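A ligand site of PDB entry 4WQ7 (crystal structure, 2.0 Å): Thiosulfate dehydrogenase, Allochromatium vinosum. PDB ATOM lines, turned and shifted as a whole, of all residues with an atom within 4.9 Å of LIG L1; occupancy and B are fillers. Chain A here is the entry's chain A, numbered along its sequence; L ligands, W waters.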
ATOM      1  N   LEU A  32     -29.314   8.044   5.729  1.00  0.00           N
ATOM      2  CA  LEU A  32     -27.866   7.862   5.781  1.00  0.00           C
ATOM      3  C   LEU A  32     -27.124   9.161   6.130  1.00  0.00           C
ATOM      4  O   LEU A  32     -26.029   9.114   6.697  1.00  0.00           O
ATOM      5  CB  LEU A  32     -27.356   7.348   4.450  1.00  0.00           C
ATOM      6  CG  LEU A  32     -27.863   5.959   4.097  1.00  0.00           C
ATOM      7  CD1 LEU A  32     -27.536   5.738   2.643  1.00  0.00           C
ATOM      8  CD2 LEU A  32     -27.196   4.909   4.945  1.00  0.00           C
ATOM      9  N   THR A  35     -29.010  10.401  10.291  1.00  0.00           N
ATOM     10  CA  THR A  35     -29.495   9.209  10.979  1.00  0.00           C
ATOM     11  C   THR A  35     -29.982   9.416  12.423  1.00  0.00           C
ATOM     12  O   THR A  35     -31.061   8.929  12.781  1.00  0.00           O
ATOM     13  CB  THR A  35     -28.431   8.131  11.019  1.00  0.00           C
ATOM     14  OG1 THR A  35     -27.551   8.272   9.887  1.00  0.00           O
ATOM     15  CG2 THR A  35     -29.114   6.787  11.007  1.00  0.00           C
ATOM     16  N   LEU A  47     -23.606  10.054  15.774  1.00  0.00           N
ATOM     17  CA  LEU A  47     -23.126   9.833  14.416  1.00  0.00           C
ATOM     18  C   LEU A  47     -24.189   9.509  13.374  1.00  0.00           C
ATOM     19  O   LEU A  47     -25.152   8.781  13.608  1.00  0.00           O
ATOM     20  CB  LEU A  47     -22.069   8.726  14.423  1.00  0.00           C
ATOM     21  CG  LEU A  47     -20.845   8.984  15.309  1.00  0.00           C
ATOM     22  CD1 LEU A  47     -19.827   7.888  15.181  1.00  0.00           C
ATOM     23  CD2 LEU A  47     -20.202  10.291  14.955  1.00  0.00           C
ATOM     24  N   ALA A  48     -23.999  10.067  12.185  1.00  0.00           N
ATOM     25  CA  ALA A  48     -24.743   9.659  11.013  1.00  0.00           C
ATOM     26  C   ALA A  48     -23.851   8.792  10.151  1.00  0.00           C
ATOM     27  O   ALA A  48     -22.644   8.841  10.300  1.00  0.00           O
ATOM     28  CB  ALA A  48     -25.214  10.846  10.233  1.00  0.00           C
ATOM     29  N   CYS A  49     -24.453   7.999   9.260  1.00  0.00           N
ATOM     30  CA  CYS A  49     -23.656   7.134   8.415  1.00  0.00           C
ATOM     31  C   CYS A  49     -22.620   7.931   7.630  1.00  0.00           C
ATOM     32  O   CYS A  49     -21.453   7.520   7.513  1.00  0.00           O
ATOM     33  CB  CYS A  49     -24.535   6.343   7.451  1.00  0.00           C
ATOM     34  SG  CYS A  49     -25.931   5.537   8.219  1.00  0.00           S
ATOM     35  N   HIS A  51     -20.776  10.276   8.433  1.00  0.00           N
ATOM     36  CA  HIS A  51     -19.586  10.739   9.156  1.00  0.00           C
ATOM     37  C   HIS A  51     -18.381   9.814   8.956  1.00  0.00           C
ATOM     38  O   HIS A  51     -17.255  10.225   9.191  1.00  0.00           O
ATOM     39  CB  HIS A  51     -19.882  10.871  10.634  1.00  0.00           C
ATOM     40  CG  HIS A  51     -20.752  12.035  10.951  1.00  0.00           C
ATOM     41  ND1 HIS A  51     -21.812  11.946  11.830  1.00  0.00           N
ATOM     42  CD2 HIS A  51     -20.695  13.318  10.543  1.00  0.00           C
ATOM     43  CE1 HIS A  51     -22.390  13.135  11.921  1.00  0.00           C
ATOM     44  NE2 HIS A  51     -21.722  13.985  11.150  1.00  0.00           N
ATOM     45  N   CYS A  52     -18.608   8.570   8.545  1.00  0.00           N
ATOM     46  CA  CYS A  52     -17.503   7.686   8.159  1.00  0.00           C
ATOM     47  C   CYS A  52     -17.633   7.231   6.704  1.00  0.00           C
ATOM     48  O   CYS A  52     -16.698   6.654   6.156  1.00  0.00           O
ATOM     49  CB  CYS A  52     -17.446   6.469   9.050  1.00  0.00           C
ATOM     50  SG  CYS A  52     -17.219   6.877  10.782  1.00  0.00           S
ATOM     51  N   HIS A  53     -18.797   7.480   6.115  1.00  0.00           N
ATOM     52  CA  HIS A  53     -19.049   7.114   4.727  1.00  0.00           C
ATOM     53  C   HIS A  53     -19.414   8.390   3.931  1.00  0.00           C
ATOM     54  O   HIS A  53     -20.541   8.547   3.472  1.00  0.00           O
ATOM     55  CB  HIS A  53     -20.183   6.078   4.641  1.00  0.00           C
ATOM     56  CG  HIS A  53     -19.915   4.780   5.356  1.00  0.00           C
ATOM     57  ND1 HIS A  53     -19.234   3.740   4.771  1.00  0.00           N
ATOM     58  CD2 HIS A  53     -20.325   4.330   6.571  1.00  0.00           C
ATOM     59  CE1 HIS A  53     -19.199   2.717   5.608  1.00  0.00           C
ATOM     60  NE2 HIS A  53     -19.841   3.053   6.713  1.00  0.00           N
ATOM     61  N   ALA A  67     -14.957   3.774   2.608  1.00  0.00           N
ATOM     62  CA  ALA A  67     -15.995   2.757   2.510  1.00  0.00           C
ATOM     63  C   ALA A  67     -17.202   3.203   1.705  1.00  0.00           C
ATOM     64  O   ALA A  67     -18.315   3.286   2.227  1.00  0.00           O
ATOM     65  CB  ALA A  67     -16.426   2.313   3.912  1.00  0.00           C
ATOM     66  N   PRO A  68     -16.984   3.495   0.408  1.00  0.00           N
ATOM     67  CA  PRO A  68     -18.103   3.894  -0.439  1.00  0.00           C
ATOM     68  C   PRO A  68     -19.116   2.766  -0.534  1.00  0.00           C
ATOM     69  O   PRO A  68     -18.741   1.593  -0.421  1.00  0.00           O
ATOM     70  CB  PRO A  68     -17.415   4.191  -1.774  1.00  0.00           C
ATOM     71  CG  PRO A  68     -16.261   3.222  -1.801  1.00  0.00           C
ATOM     72  CD  PRO A  68     -15.753   3.259  -0.371  1.00  0.00           C
ATOM     73  N   PHE A  69     -20.387   3.119  -0.695  1.00  0.00           N
ATOM     74  CA  PHE A  69     -21.455   2.151  -0.916  1.00  0.00           C
ATOM     75  C   PHE A  69     -21.619   1.769  -2.387  1.00  0.00           C
ATOM     76  O   PHE A  69     -22.382   0.859  -2.717  1.00  0.00           O
ATOM     77  CB  PHE A  69     -22.783   2.682  -0.400  1.00  0.00           C
ATOM     78  CG  PHE A  69     -22.800   2.963   1.089  1.00  0.00           C
ATOM     79  CD1 PHE A  69     -22.216   2.079   1.981  1.00  0.00           C
ATOM     80  CD2 PHE A  69     -23.422   4.090   1.584  1.00  0.00           C
ATOM     81  CE1 PHE A  69     -22.236   2.351   3.339  1.00  0.00           C
ATOM     82  CE2 PHE A  69     -23.447   4.338   2.946  1.00  0.00           C
ATOM     83  CZ  PHE A  69     -22.862   3.463   3.818  1.00  0.00           C
ATOM     84  N   VAL A  72     -21.589  -1.915  -3.367  1.00  0.00           N
ATOM     85  CA  VAL A  72     -21.653  -2.777  -2.181  1.00  0.00           C
ATOM     86  C   VAL A  72     -22.681  -3.907  -2.307  1.00  0.00           C
ATOM     87  O   VAL A  72     -22.448  -5.013  -1.806  1.00  0.00           O
ATOM     88  CB  VAL A  72     -21.923  -1.945  -0.897  1.00  0.00           C
ATOM     89  CG1 VAL A  72     -23.355  -1.404  -0.854  1.00  0.00           C
ATOM     90  CG2 VAL A  72     -21.660  -2.770   0.305  1.00  0.00           C
ATOM     91  N   PHE A  76     -22.559  -8.857  -1.362  1.00  0.00           N
ATOM     92  CA  PHE A  76     -23.261  -9.584  -0.307  1.00  0.00           C
ATOM     93  C   PHE A  76     -24.259 -10.579  -0.925  1.00  0.00           C
ATOM     94  O   PHE A  76     -24.767 -10.333  -2.008  1.00  0.00           O
ATOM     95  CB  PHE A  76     -24.000  -8.620   0.625  1.00  0.00           C
ATOM     96  CG  PHE A  76     -23.085  -7.889   1.527  1.00  0.00           C
ATOM     97  CD1 PHE A  76     -22.864  -8.340   2.804  1.00  0.00           C
ATOM     98  CD2 PHE A  76     -22.405  -6.788   1.082  1.00  0.00           C
ATOM     99  CE1 PHE A  76     -21.983  -7.687   3.625  1.00  0.00           C
ATOM    100  CE2 PHE A  76     -21.539  -6.117   1.909  1.00  0.00           C
ATOM    101  CZ  PHE A  76     -21.331  -6.571   3.179  1.00  0.00           C
ATOM    102  N   GLN A  78     -21.894 -12.460   2.145  1.00  0.00           N
ATOM    103  CA  GLN A  78     -20.470 -12.701   2.218  1.00  0.00           C
ATOM    104  C   GLN A  78     -20.186 -13.214   3.610  1.00  0.00           C
ATOM    105  O   GLN A  78     -20.967 -13.010   4.552  1.00  0.00           O
ATOM    106  CB  GLN A  78     -19.655 -11.437   1.904  1.00  0.00           C
ATOM    107  CG  GLN A  78     -19.711 -10.423   3.041  1.00  0.00           C
ATOM    108  CD  GLN A  78     -18.937  -9.138   2.801  1.00  0.00           C
ATOM    109  OE1 GLN A  78     -18.375  -8.578   3.739  1.00  0.00           O
ATOM    110  NE2 GLN A  78     -18.928  -8.657   1.578  1.00  0.00           N
ATOM    111  N   LEU A  89     -26.405  -7.932   3.328  1.00  0.00           N
ATOM    112  CA  LEU A  89     -26.191  -6.481   3.471  1.00  0.00           C
ATOM    113  C   LEU A  89     -27.046  -5.866   4.595  1.00  0.00           C
ATOM    114  O   LEU A  89     -26.580  -4.976   5.324  1.00  0.00           O
ATOM    115  CB  LEU A  89     -26.499  -5.772   2.152  1.00  0.00           C
ATOM    116  CG  LEU A  89     -26.256  -4.273   2.089  1.00  0.00           C
ATOM    117  CD1 LEU A  89     -24.848  -3.880   2.605  1.00  0.00           C
ATOM    118  CD2 LEU A  89     -26.471  -3.871   0.654  1.00  0.00           C
ATOM    119  N   ARG A  92     -25.265  -6.491   7.696  1.00  0.00           N
ATOM    120  CA  ARG A  92     -24.076  -5.652   7.784  1.00  0.00           C
ATOM    121  C   ARG A  92     -24.469  -4.240   8.232  1.00  0.00           C
ATOM    122  O   ARG A  92     -23.809  -3.642   9.093  1.00  0.00           O
ATOM    123  CB  ARG A  92     -23.314  -5.628   6.435  1.00  0.00           C
ATOM    124  CG  ARG A  92     -22.039  -4.770   6.471  1.00  0.00           C
ATOM    125  CD  ARG A  92     -21.082  -5.430   7.396  1.00  0.00           C
ATOM    126  NE  ARG A  92     -19.829  -4.729   7.655  1.00  0.00           N
ATOM    127  CZ  ARG A  92     -19.700  -3.716   8.500  1.00  0.00           C
ATOM    128  NH1 ARG A  92     -20.746  -3.210   9.134  1.00  0.00           N
ATOM    129  NH2 ARG A  92     -18.510  -3.191   8.712  1.00  0.00           N
ATOM    130  N   ILE A  93     -25.576  -3.716   7.720  1.00  0.00           N
ATOM    131  CA  ILE A  93     -26.018  -2.375   8.138  1.00  0.00           C
ATOM    132  C   ILE A  93     -26.348  -2.398   9.623  1.00  0.00           C
ATOM    133  O   ILE A  93     -25.937  -1.518  10.379  1.00  0.00           O
ATOM    134  CB  ILE A  93     -27.218  -1.918   7.304  1.00  0.00           C
ATOM    135  CG1 ILE A  93     -26.756  -1.590   5.884  1.00  0.00           C
ATOM    136  CG2 ILE A  93     -27.933  -0.707   7.974  1.00  0.00           C
ATOM    137  CD1 ILE A  93     -27.871  -1.381   4.896  1.00  0.00           C
ATOM    138  N   CYS A  96     -23.381  -1.878  11.792  1.00  0.00           N
ATOM    139  CA  CYS A  96     -22.852  -0.518  11.953  1.00  0.00           C
ATOM    140  C   CYS A  96     -23.816   0.276  12.865  1.00  0.00           C
ATOM    141  O   CYS A  96     -23.384   1.156  13.598  1.00  0.00           O
ATOM    142  CB  CYS A  96     -22.610   0.172  10.611  1.00  0.00           C
ATOM    143  SG  CYS A  96     -20.780   0.126  10.007  1.00  0.00           S
ATOM    144  N   PHE A  97     -25.109  -0.052  12.857  1.00  0.00           N
ATOM    145  CA  PHE A  97     -26.030   0.560  13.826  1.00  0.00           C
ATOM    146  C   PHE A  97     -25.629   0.223  15.261  1.00  0.00           C
ATOM    147  O   PHE A  97     -25.600   1.083  16.124  1.00  0.00           O
ATOM    148  CB  PHE A  97     -27.481   0.148  13.596  1.00  0.00           C
ATOM    149  CG  PHE A  97     -28.255   1.069  12.698  1.00  0.00           C
ATOM    150  CD1 PHE A  97     -28.925   2.181  13.221  1.00  0.00           C
ATOM    151  CD2 PHE A  97     -28.340   0.821  11.321  1.00  0.00           C
ATOM    152  CE1 PHE A  97     -29.634   3.020  12.401  1.00  0.00           C
ATOM    153  CE2 PHE A  97     -29.063   1.685  10.487  1.00  0.00           C
ATOM    154  CZ  PHE A  97     -29.699   2.785  11.027  1.00  0.00           C
ATOM    155  N   SER A 100     -20.913   1.252  15.264  1.00  0.00           N
ATOM    156  CA  SER A 100     -20.565   2.591  14.867  1.00  0.00           C
ATOM    157  C   SER A 100     -21.551   3.648  15.377  1.00  0.00           C
ATOM    158  O   SER A 100     -21.132   4.773  15.687  1.00  0.00           O
ATOM    159  CB  SER A 100     -20.494   2.678  13.366  1.00  0.00           C
ATOM    160  OG  SER A 100     -19.554   1.760  12.892  1.00  0.00           O
ATOM    161  N   LEU A 101     -22.838   3.293  15.495  1.00  0.00           N
ATOM    162  CA  LEU A 101     -23.834   4.221  16.032  1.00  0.00           C
ATOM    163  C   LEU A 101     -24.309   3.847  17.436  1.00  0.00           C
ATOM    164  O   LEU A 101     -25.269   4.428  17.924  1.00  0.00           O
ATOM    165  CB  LEU A 101     -25.062   4.300  15.130  1.00  0.00           C
ATOM    166  CG  LEU A 101     -24.902   4.731  13.678  1.00  0.00           C
ATOM    167  CD1 LEU A 101     -26.216   5.310  13.165  1.00  0.00           C
ATOM    168  CD2 LEU A 101     -23.830   5.675  13.513  1.00  0.00           C
ATOM    169  N   MET A 116     -32.676   2.506   2.739  1.00  0.00           N
ATOM    170  CA  MET A 116     -31.223   2.558   2.677  1.00  0.00           C
ATOM    171  C   MET A 116     -30.668   1.557   1.658  1.00  0.00           C
ATOM    172  O   MET A 116     -29.742   1.874   0.925  1.00  0.00           O
ATOM    173  CB  MET A 116     -30.627   2.300   4.051  1.00  0.00           C
ATOM    174  CG  MET A 116     -30.760   3.452   5.080  1.00  0.00           C
ATOM    175  SD  MET A 116     -30.102   2.840   6.674  1.00  0.00           S
ATOM    176  CE  MET A 116     -29.828   4.310   7.657  1.00  0.00           C
ATOM    177  N   MET A 120     -28.433   2.374  -1.709  1.00  0.00           N
ATOM    178  CA  MET A 120     -27.196   1.678  -2.066  1.00  0.00           C
ATOM    179  C   MET A 120     -27.297   0.932  -3.400  1.00  0.00           C
ATOM    180  O   MET A 120     -26.309   0.848  -4.144  1.00  0.00           O
ATOM    181  CB  MET A 120     -26.788   0.692  -0.955  1.00  0.00           C
ATOM    182  CG  MET A 120     -26.542   1.361   0.364  1.00  0.00           C
ATOM    183  SD  MET A 120     -26.002   0.217   1.668  1.00  0.00           S
ATOM    184  CE  MET A 120     -26.035   1.238   3.099  1.00  0.00           C
ATOM    185  N   GLY A 137     -14.134  -0.079   0.653  1.00  0.00           N
ATOM    186  CA  GLY A 137     -13.618  -0.248   2.000  1.00  0.00           C
ATOM    187  C   GLY A 137     -12.789   0.928   2.490  1.00  0.00           C
ATOM    188  O   GLY A 137     -12.770   2.033   1.908  1.00  0.00           O
ATOM    189  N   ILE A 138     -12.119   0.695   3.608  1.00  0.00           N
ATOM    190  CA  ILE A 138     -11.118   1.592   4.149  1.00  0.00           C
ATOM    191  C   ILE A 138      -9.819   0.813   4.183  1.00  0.00           C
ATOM    192  O   ILE A 138      -9.653  -0.057   5.019  1.00  0.00           O
ATOM    193  CB  ILE A 138     -11.483   2.090   5.569  1.00  0.00           C
ATOM    194  CG1 ILE A 138     -12.705   2.988   5.486  1.00  0.00           C
ATOM    195  CG2 ILE A 138     -10.304   2.832   6.225  1.00  0.00           C
ATOM    196  CD1 ILE A 138     -13.453   3.038   6.741  1.00  0.00           C
ATOM    197  N   PHE A 189     -18.387   6.562  18.427  1.00  0.00           N
ATOM    198  CA  PHE A 189     -18.539   5.149  18.140  1.00  0.00           C
ATOM    199  C   PHE A 189     -18.084   4.281  19.336  1.00  0.00           C
ATOM    200  O   PHE A 189     -17.290   4.721  20.135  1.00  0.00           O
ATOM    201  CB  PHE A 189     -17.769   4.813  16.851  1.00  0.00           C
ATOM    202  CG  PHE A 189     -16.261   5.104  16.867  1.00  0.00           C
ATOM    203  CD1 PHE A 189     -15.367   4.217  17.444  1.00  0.00           C
ATOM    204  CD2 PHE A 189     -15.737   6.203  16.207  1.00  0.00           C
ATOM    205  CE1 PHE A 189     -14.015   4.446  17.420  1.00  0.00           C
ATOM    206  CE2 PHE A 189     -14.381   6.446  16.199  1.00  0.00           C
ATOM    207  CZ  PHE A 189     -13.509   5.560  16.798  1.00  0.00           C
ATOM    208  N   GLY A 194     -15.372  -0.831  13.764  1.00  0.00           N
ATOM    209  CA  GLY A 194     -14.146  -1.041  13.011  1.00  0.00           C
ATOM    210  C   GLY A 194     -13.206   0.152  13.171  1.00  0.00           C
ATOM    211  O   GLY A 194     -11.978   0.025  13.133  1.00  0.00           O
ATOM    212  N   MET A 195     -13.790   1.327  13.348  1.00  0.00           N
ATOM    213  CA  MET A 195     -13.000   2.539  13.498  1.00  0.00           C
ATOM    214  C   MET A 195     -12.222   2.545  14.817  1.00  0.00           C
ATOM    215  O   MET A 195     -11.313   3.361  15.012  1.00  0.00           O
ATOM    216  CB  MET A 195     -13.923   3.746  13.400  1.00  0.00           C
ATOM    217  CG  MET A 195     -13.216   5.056  13.175  1.00  0.00           C
ATOM    218  SD  MET A 195     -12.402   5.153  11.544  1.00  0.00           S
ATOM    219  CE  MET A 195     -13.752   5.241  10.366  1.00  0.00           C
ATOM    220  N   THR A 200      -7.290   0.549  10.891  1.00  0.00           N
ATOM    221  CA  THR A 200      -8.447   1.085  10.178  1.00  0.00           C
ATOM    222  C   THR A 200      -8.558   2.584  10.406  1.00  0.00           C
ATOM    223  O   THR A 200      -8.711   3.345   9.450  1.00  0.00           O
ATOM    224  CB  THR A 200      -9.744   0.382  10.603  1.00  0.00           C
ATOM    225  OG1 THR A 200      -9.690  -0.984  10.208  1.00  0.00           O
ATOM    226  CG2 THR A 200     -10.969   0.985   9.948  1.00  0.00           C
HETATM  227 FE1  LIG L   1     -20.328   1.687   8.224  1.00  0.00          FE
HETATM  228  C1  LIG L   1     -18.489  -0.831   6.640  1.00  0.00           C
HETATM  229  C2  LIG L   1     -23.127   0.792   6.388  1.00  0.00           C
HETATM  230  C3  LIG L   1     -22.140   4.129   9.866  1.00  0.00           C
HETATM  231  C4  LIG L   1     -17.382   2.775   9.785  1.00  0.00           C
HETATM  232  N1  LIG L   1     -20.745   0.245   6.771  1.00  0.00           N
HETATM  233  C5  LIG L   1     -19.889  -0.642   6.269  1.00  0.00           C
HETATM  234  C6  LIG L   1     -20.480  -1.515   5.252  1.00  0.00           C
HETATM  235  C7  LIG L   1     -21.866  -1.049   5.153  1.00  0.00           C
HETATM  236  C8  LIG L   1     -21.896   0.067   6.151  1.00  0.00           C
HETATM  237  C9  LIG L   1     -22.972  -1.555   4.282  1.00  0.00           C
HETATM  238  C10 LIG L   1     -19.783  -2.601   4.492  1.00  0.00           C
HETATM  239  C11 LIG L   1     -19.073  -1.924   3.304  1.00  0.00           C
HETATM  240  C12 LIG L   1     -18.359  -2.933   2.418  1.00  0.00           C
HETATM  241  O1  LIG L   1     -18.482  -4.144   2.641  1.00  0.00           O
HETATM  242  O2  LIG L   1     -17.687  -2.534   1.443  1.00  0.00           O
HETATM  243  N2  LIG L   1     -22.292   2.317   8.150  1.00  0.00           N
HETATM  244  C13 LIG L   1     -23.232   1.844   7.367  1.00  0.00           C
HETATM  245  C14 LIG L   1     -24.525   2.512   7.535  1.00  0.00           C
HETATM  246  C15 LIG L   1     -24.256   3.494   8.581  1.00  0.00           C
HETATM  247  C16 LIG L   1     -22.819   3.282   8.886  1.00  0.00           C
HETATM  248  C17 LIG L   1     -25.779   2.216   6.811  1.00  0.00           C
HETATM  249  C18 LIG L   1     -25.190   4.470   9.232  1.00  0.00           C
HETATM  250  C19 LIG L   1     -26.261   3.640   9.921  1.00  0.00           C
HETATM  251  N3  LIG L   1     -19.854   3.185   9.604  1.00  0.00           N
HETATM  252  C20 LIG L   1     -20.699   4.059  10.122  1.00  0.00           C
HETATM  253  C21 LIG L   1     -20.023   5.058  10.991  1.00  0.00           C
HETATM  254  C22 LIG L   1     -18.614   4.626  10.969  1.00  0.00           C
HETATM  255  C23 LIG L   1     -18.646   3.460  10.066  1.00  0.00           C
HETATM  256  C24 LIG L   1     -20.681   6.192  11.735  1.00  0.00           C
HETATM  257  C25 LIG L   1     -17.397   5.216  11.651  1.00  0.00           C
HETATM  258  C26 LIG L   1     -17.650   5.368  13.122  1.00  0.00           C
HETATM  259  N4  LIG L   1     -18.319   1.088   8.214  1.00  0.00           N
HETATM  260  C27 LIG L   1     -17.326   1.623   8.911  1.00  0.00           C
HETATM  261  C28 LIG L   1     -16.019   0.945   8.725  1.00  0.00           C
HETATM  262  C29 LIG L   1     -16.354  -0.134   7.798  1.00  0.00           C
HETATM  263  C30 LIG L   1     -17.796   0.059   7.566  1.00  0.00           C
HETATM  264  C31 LIG L   1     -14.679   1.270   9.352  1.00  0.00           C
HETATM  265  C32 LIG L   1     -15.436  -1.177   7.229  1.00  0.00           C
HETATM  266  C33 LIG L   1     -14.867  -0.729   5.904  1.00  0.00           C
HETATM  267  C34 LIG L   1     -14.116  -1.871   5.232  1.00  0.00           C
HETATM  268  O3  LIG L   1     -14.769  -2.898   4.906  1.00  0.00           O
HETATM  269  O4  LIG L   1     -12.896  -1.743   5.021  1.00  0.00           O
HETATM  270 FE1  LG2 L   2     -11.961  14.572  10.974  1.00  0.00          FE
HETATM  271  C1  LG2 L   2     -14.644  12.524  10.239  1.00  0.00           C
HETATM  272  C2  LG2 L   2     -10.347  12.056  12.695  1.00  0.00           C
HETATM  273  C3  LG2 L   2      -9.027  16.524  11.167  1.00  0.00           C
HETATM  274  C4  LG2 L   2     -13.695  17.343   9.807  1.00  0.00           C
HETATM  275  N1  LG2 L   2     -12.423  12.606  11.402  1.00  0.00           N
HETATM  276  C5  LG2 L   2     -13.535  11.977  11.050  1.00  0.00           C
HETATM  277  C6  LG2 L   2     -13.542  10.586  11.558  1.00  0.00           C
HETATM  278  C7  LG2 L   2     -12.279  10.459  12.295  1.00  0.00           C
HETATM  279  C8  LG2 L   2     -11.656  11.788  12.119  1.00  0.00           C
HETATM  280  C9  LG2 L   2     -11.758   9.273  13.022  1.00  0.00           C
HETATM  281  C10 LG2 L   2     -14.613   9.531  11.445  1.00  0.00           C
HETATM  282  C11 LG2 L   2     -15.826  10.026  12.274  1.00  0.00           C
HETATM  283  C12 LG2 L   2     -15.751   9.985  13.808  1.00  0.00           C
HETATM  284  O1  LG2 L   2     -14.968   9.222  14.394  1.00  0.00           O
HETATM  285  O2  LG2 L   2     -16.537  10.699  14.501  1.00  0.00           O
HETATM  286  N2  LG2 L   2     -10.041  14.342  11.755  1.00  0.00           N
HETATM  287  C13 LG2 L   2      -9.610  13.289  12.424  1.00  0.00           C
HETATM  288  C14 LG2 L   2      -8.200  13.408  12.851  1.00  0.00           C
HETATM  289  C15 LG2 L   2      -7.793  14.730  12.379  1.00  0.00           C
HETATM  290  C16 LG2 L   2      -9.018  15.194  11.707  1.00  0.00           C
HETATM  291  C17 LG2 L   2      -7.433  12.398  13.588  1.00  0.00           C
HETATM  292  C18 LG2 L   2      -6.463  15.430  12.483  1.00  0.00           C
HETATM  293  C19 LG2 L   2      -5.492  14.565  11.712  1.00  0.00           C
HETATM  294  N3  LG2 L   2     -11.456  16.540  10.570  1.00  0.00           N
HETATM  295  C20 LG2 L   2     -10.272  17.132  10.722  1.00  0.00           C
HETATM  296  C21 LG2 L   2     -10.283  18.582  10.415  1.00  0.00           C
HETATM  297  C22 LG2 L   2     -11.683  18.831  10.020  1.00  0.00           C
HETATM  298  C23 LG2 L   2     -12.304  17.489  10.171  1.00  0.00           C
HETATM  299  C24 LG2 L   2      -9.130  19.544  10.484  1.00  0.00           C
HETATM  300  C25 LG2 L   2     -12.348  20.151   9.647  1.00  0.00           C
HETATM  301  C26 LG2 L   2     -11.796  20.802   8.423  1.00  0.00           C
HETATM  302  N4  LG2 L   2     -13.843  14.865  10.145  1.00  0.00           N
HETATM  303  C27 LG2 L   2     -14.345  16.034   9.716  1.00  0.00           C
HETATM  304  C28 LG2 L   2     -15.710  15.899   9.124  1.00  0.00           C
HETATM  305  C29 LG2 L   2     -15.979  14.464   9.232  1.00  0.00           C
HETATM  306  C30 LG2 L   2     -14.755  13.927   9.878  1.00  0.00           C
HETATM  307  C31 LG2 L   2     -16.578  16.985   8.509  1.00  0.00           C
HETATM  308  C32 LG2 L   2     -17.158  13.697   8.780  1.00  0.00           C
HETATM  309  C33 LG2 L   2     -16.694  12.954   7.518  1.00  0.00           C
HETATM  310  C34 LG2 L   2     -16.543  13.827   6.266  1.00  0.00           C
HETATM  311  O3  LG2 L   2     -17.546  14.416   5.766  1.00  0.00           O
HETATM  312  O4  LG2 L   2     -15.426  13.929   5.736  1.00  0.00           O
HETATM  313  O   HOH W   1     -17.529  -6.009   1.088  1.00  0.00           O
HETATM  314  O   HOH W   2     -16.734   1.568  12.509  1.00  0.00           O
HETATM  315  O   HOH W   3     -15.190  -3.457   1.175  1.00  0.00           O
HETATM  316  O   HOH W   4     -18.301  -5.687   4.571  1.00  0.00           O
HETATM  317  O   HOH W   5     -16.871  -0.019   0.741  1.00  0.00           O
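CD2 of Leu 32 touches C17 of LIG L1, 3.6 Å away.
CD1 of Leu 47 touches C26 of LIG L1, 3.9 Å away.
Ala 48 touches LIG L1.
Ala 67 touches LIG L1.
CE1 of Phe 69 touches C2 of LIG L1 (3.5 Å).
Val 72 touches LIG L1 (CG2 to C12, 3.9 Å).
Phe 76 touches LIG L1.
CD1 of Leu 89 touches C9 of LIG L1 (3.4 Å).
Arg 92 touches LIG L1.
CG2 of Ile 93 touches C17 of LIG L1 (3.8 Å).
Phe 97 touches LIG L1.
Ser 100 touches LIG L1 (CB to C21, 3.4 Å).
CD1 of Leu 101 touches C19 of LIG L1, 3.6 Å away.
Met 120 touches LIG L1.
Gly 137 touches LIG L1 (CA to O4, 3.4 Å).
Phe 189 touches LIG L1.
Met 195 touches LIG L1.
CG2 of Thr 200 touches C31 of LIG L1 (3.8 Å).
Hydrophobic or aromatic side chains within 4 Å of LIG L1: Leu 32, Leu 47, His 53, Ala 67, Phe 69, Val 72, Phe 76, Leu 89, Ile 93, Phe 97, Leu 101, Met 120, Ile 138, Phe 189 and Met 195.
Of the 29 residues printed, 23 come within 4 Å of LIG L1.
The side-chain sulfur of Cys 49 is covalently linked to a carbon (C18) of LIG L1 (1.6 Å).
A carbon (C25) of LIG L1 is covalently linked to the side-chain sulfur (SG) of Cys 52, at 1.9 Å.
A ring nitrogen (NE2) of His 53 is bound to an iron atom (FE1) of LIG L1 (2.1 Å).
An iron atom (FE1) of LIG L1 is bound by the side-chain sulfur of Cys 96 (2.4 Å).
An oxygen (O4) of LIG L1 lies within hydrogen-bond range of the backbone NH (N) of Ile 138 (2.9 Å).
The backbone carbonyl oxygen of Leu 32 lies within hydrogen-bond range of the backbone NH of Cys 49.
N of Cys 49 is in hydrogen-bond range of OG1 of Thr 35 (3.2 Å).
ND1 of His 53 is in hydrogen-bond range of O of Ala 67.
The guanidinium group (NH1) of Arg 92 sits close to the side-chain sulfur (SG) of Cys 96.
OG of Ser 100 lies close to SG of Cys 96, at 3.5 Å.
O of Cys 96 is in hydrogen-bond range of N of Leu 101 (2.9 Å).
The backbone carbonyl oxygen (O) of Gly 137 is in hydrogen-bond range of the backbone NH (N) of Ala 67.
A ring nitrogen (ND1) of His 51 lies within hydrogen-bond range of the backbone NH (N) of Ala 48.
Water W4 lies within hydrogen-bond range of an oxygen (O1) of LIG L1 (2.5 Å) and the side-chain amide oxygen of Gln 78 (3.0 Å).
Water W1 lies within hydrogen-bond range of O1 of LIG L1 (2.6 Å) and NE2 of Gln 78 (3.0 Å).
Water W5 lies within hydrogen-bond range of the backbone carbonyl oxygen of Pro 68 (2.7 Å), an oxygen (O2) of LIG L1 (2.7 Å) and the backbone NH of Gly 137 (2.7 Å).
Water W2 lies within hydrogen-bond range of the side-chain hydroxyl of Ser 100 (2.9 Å), the backbone NH of Gly 194 (3.0 Å) and the backbone NH of Met 195 (3.1 Å).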
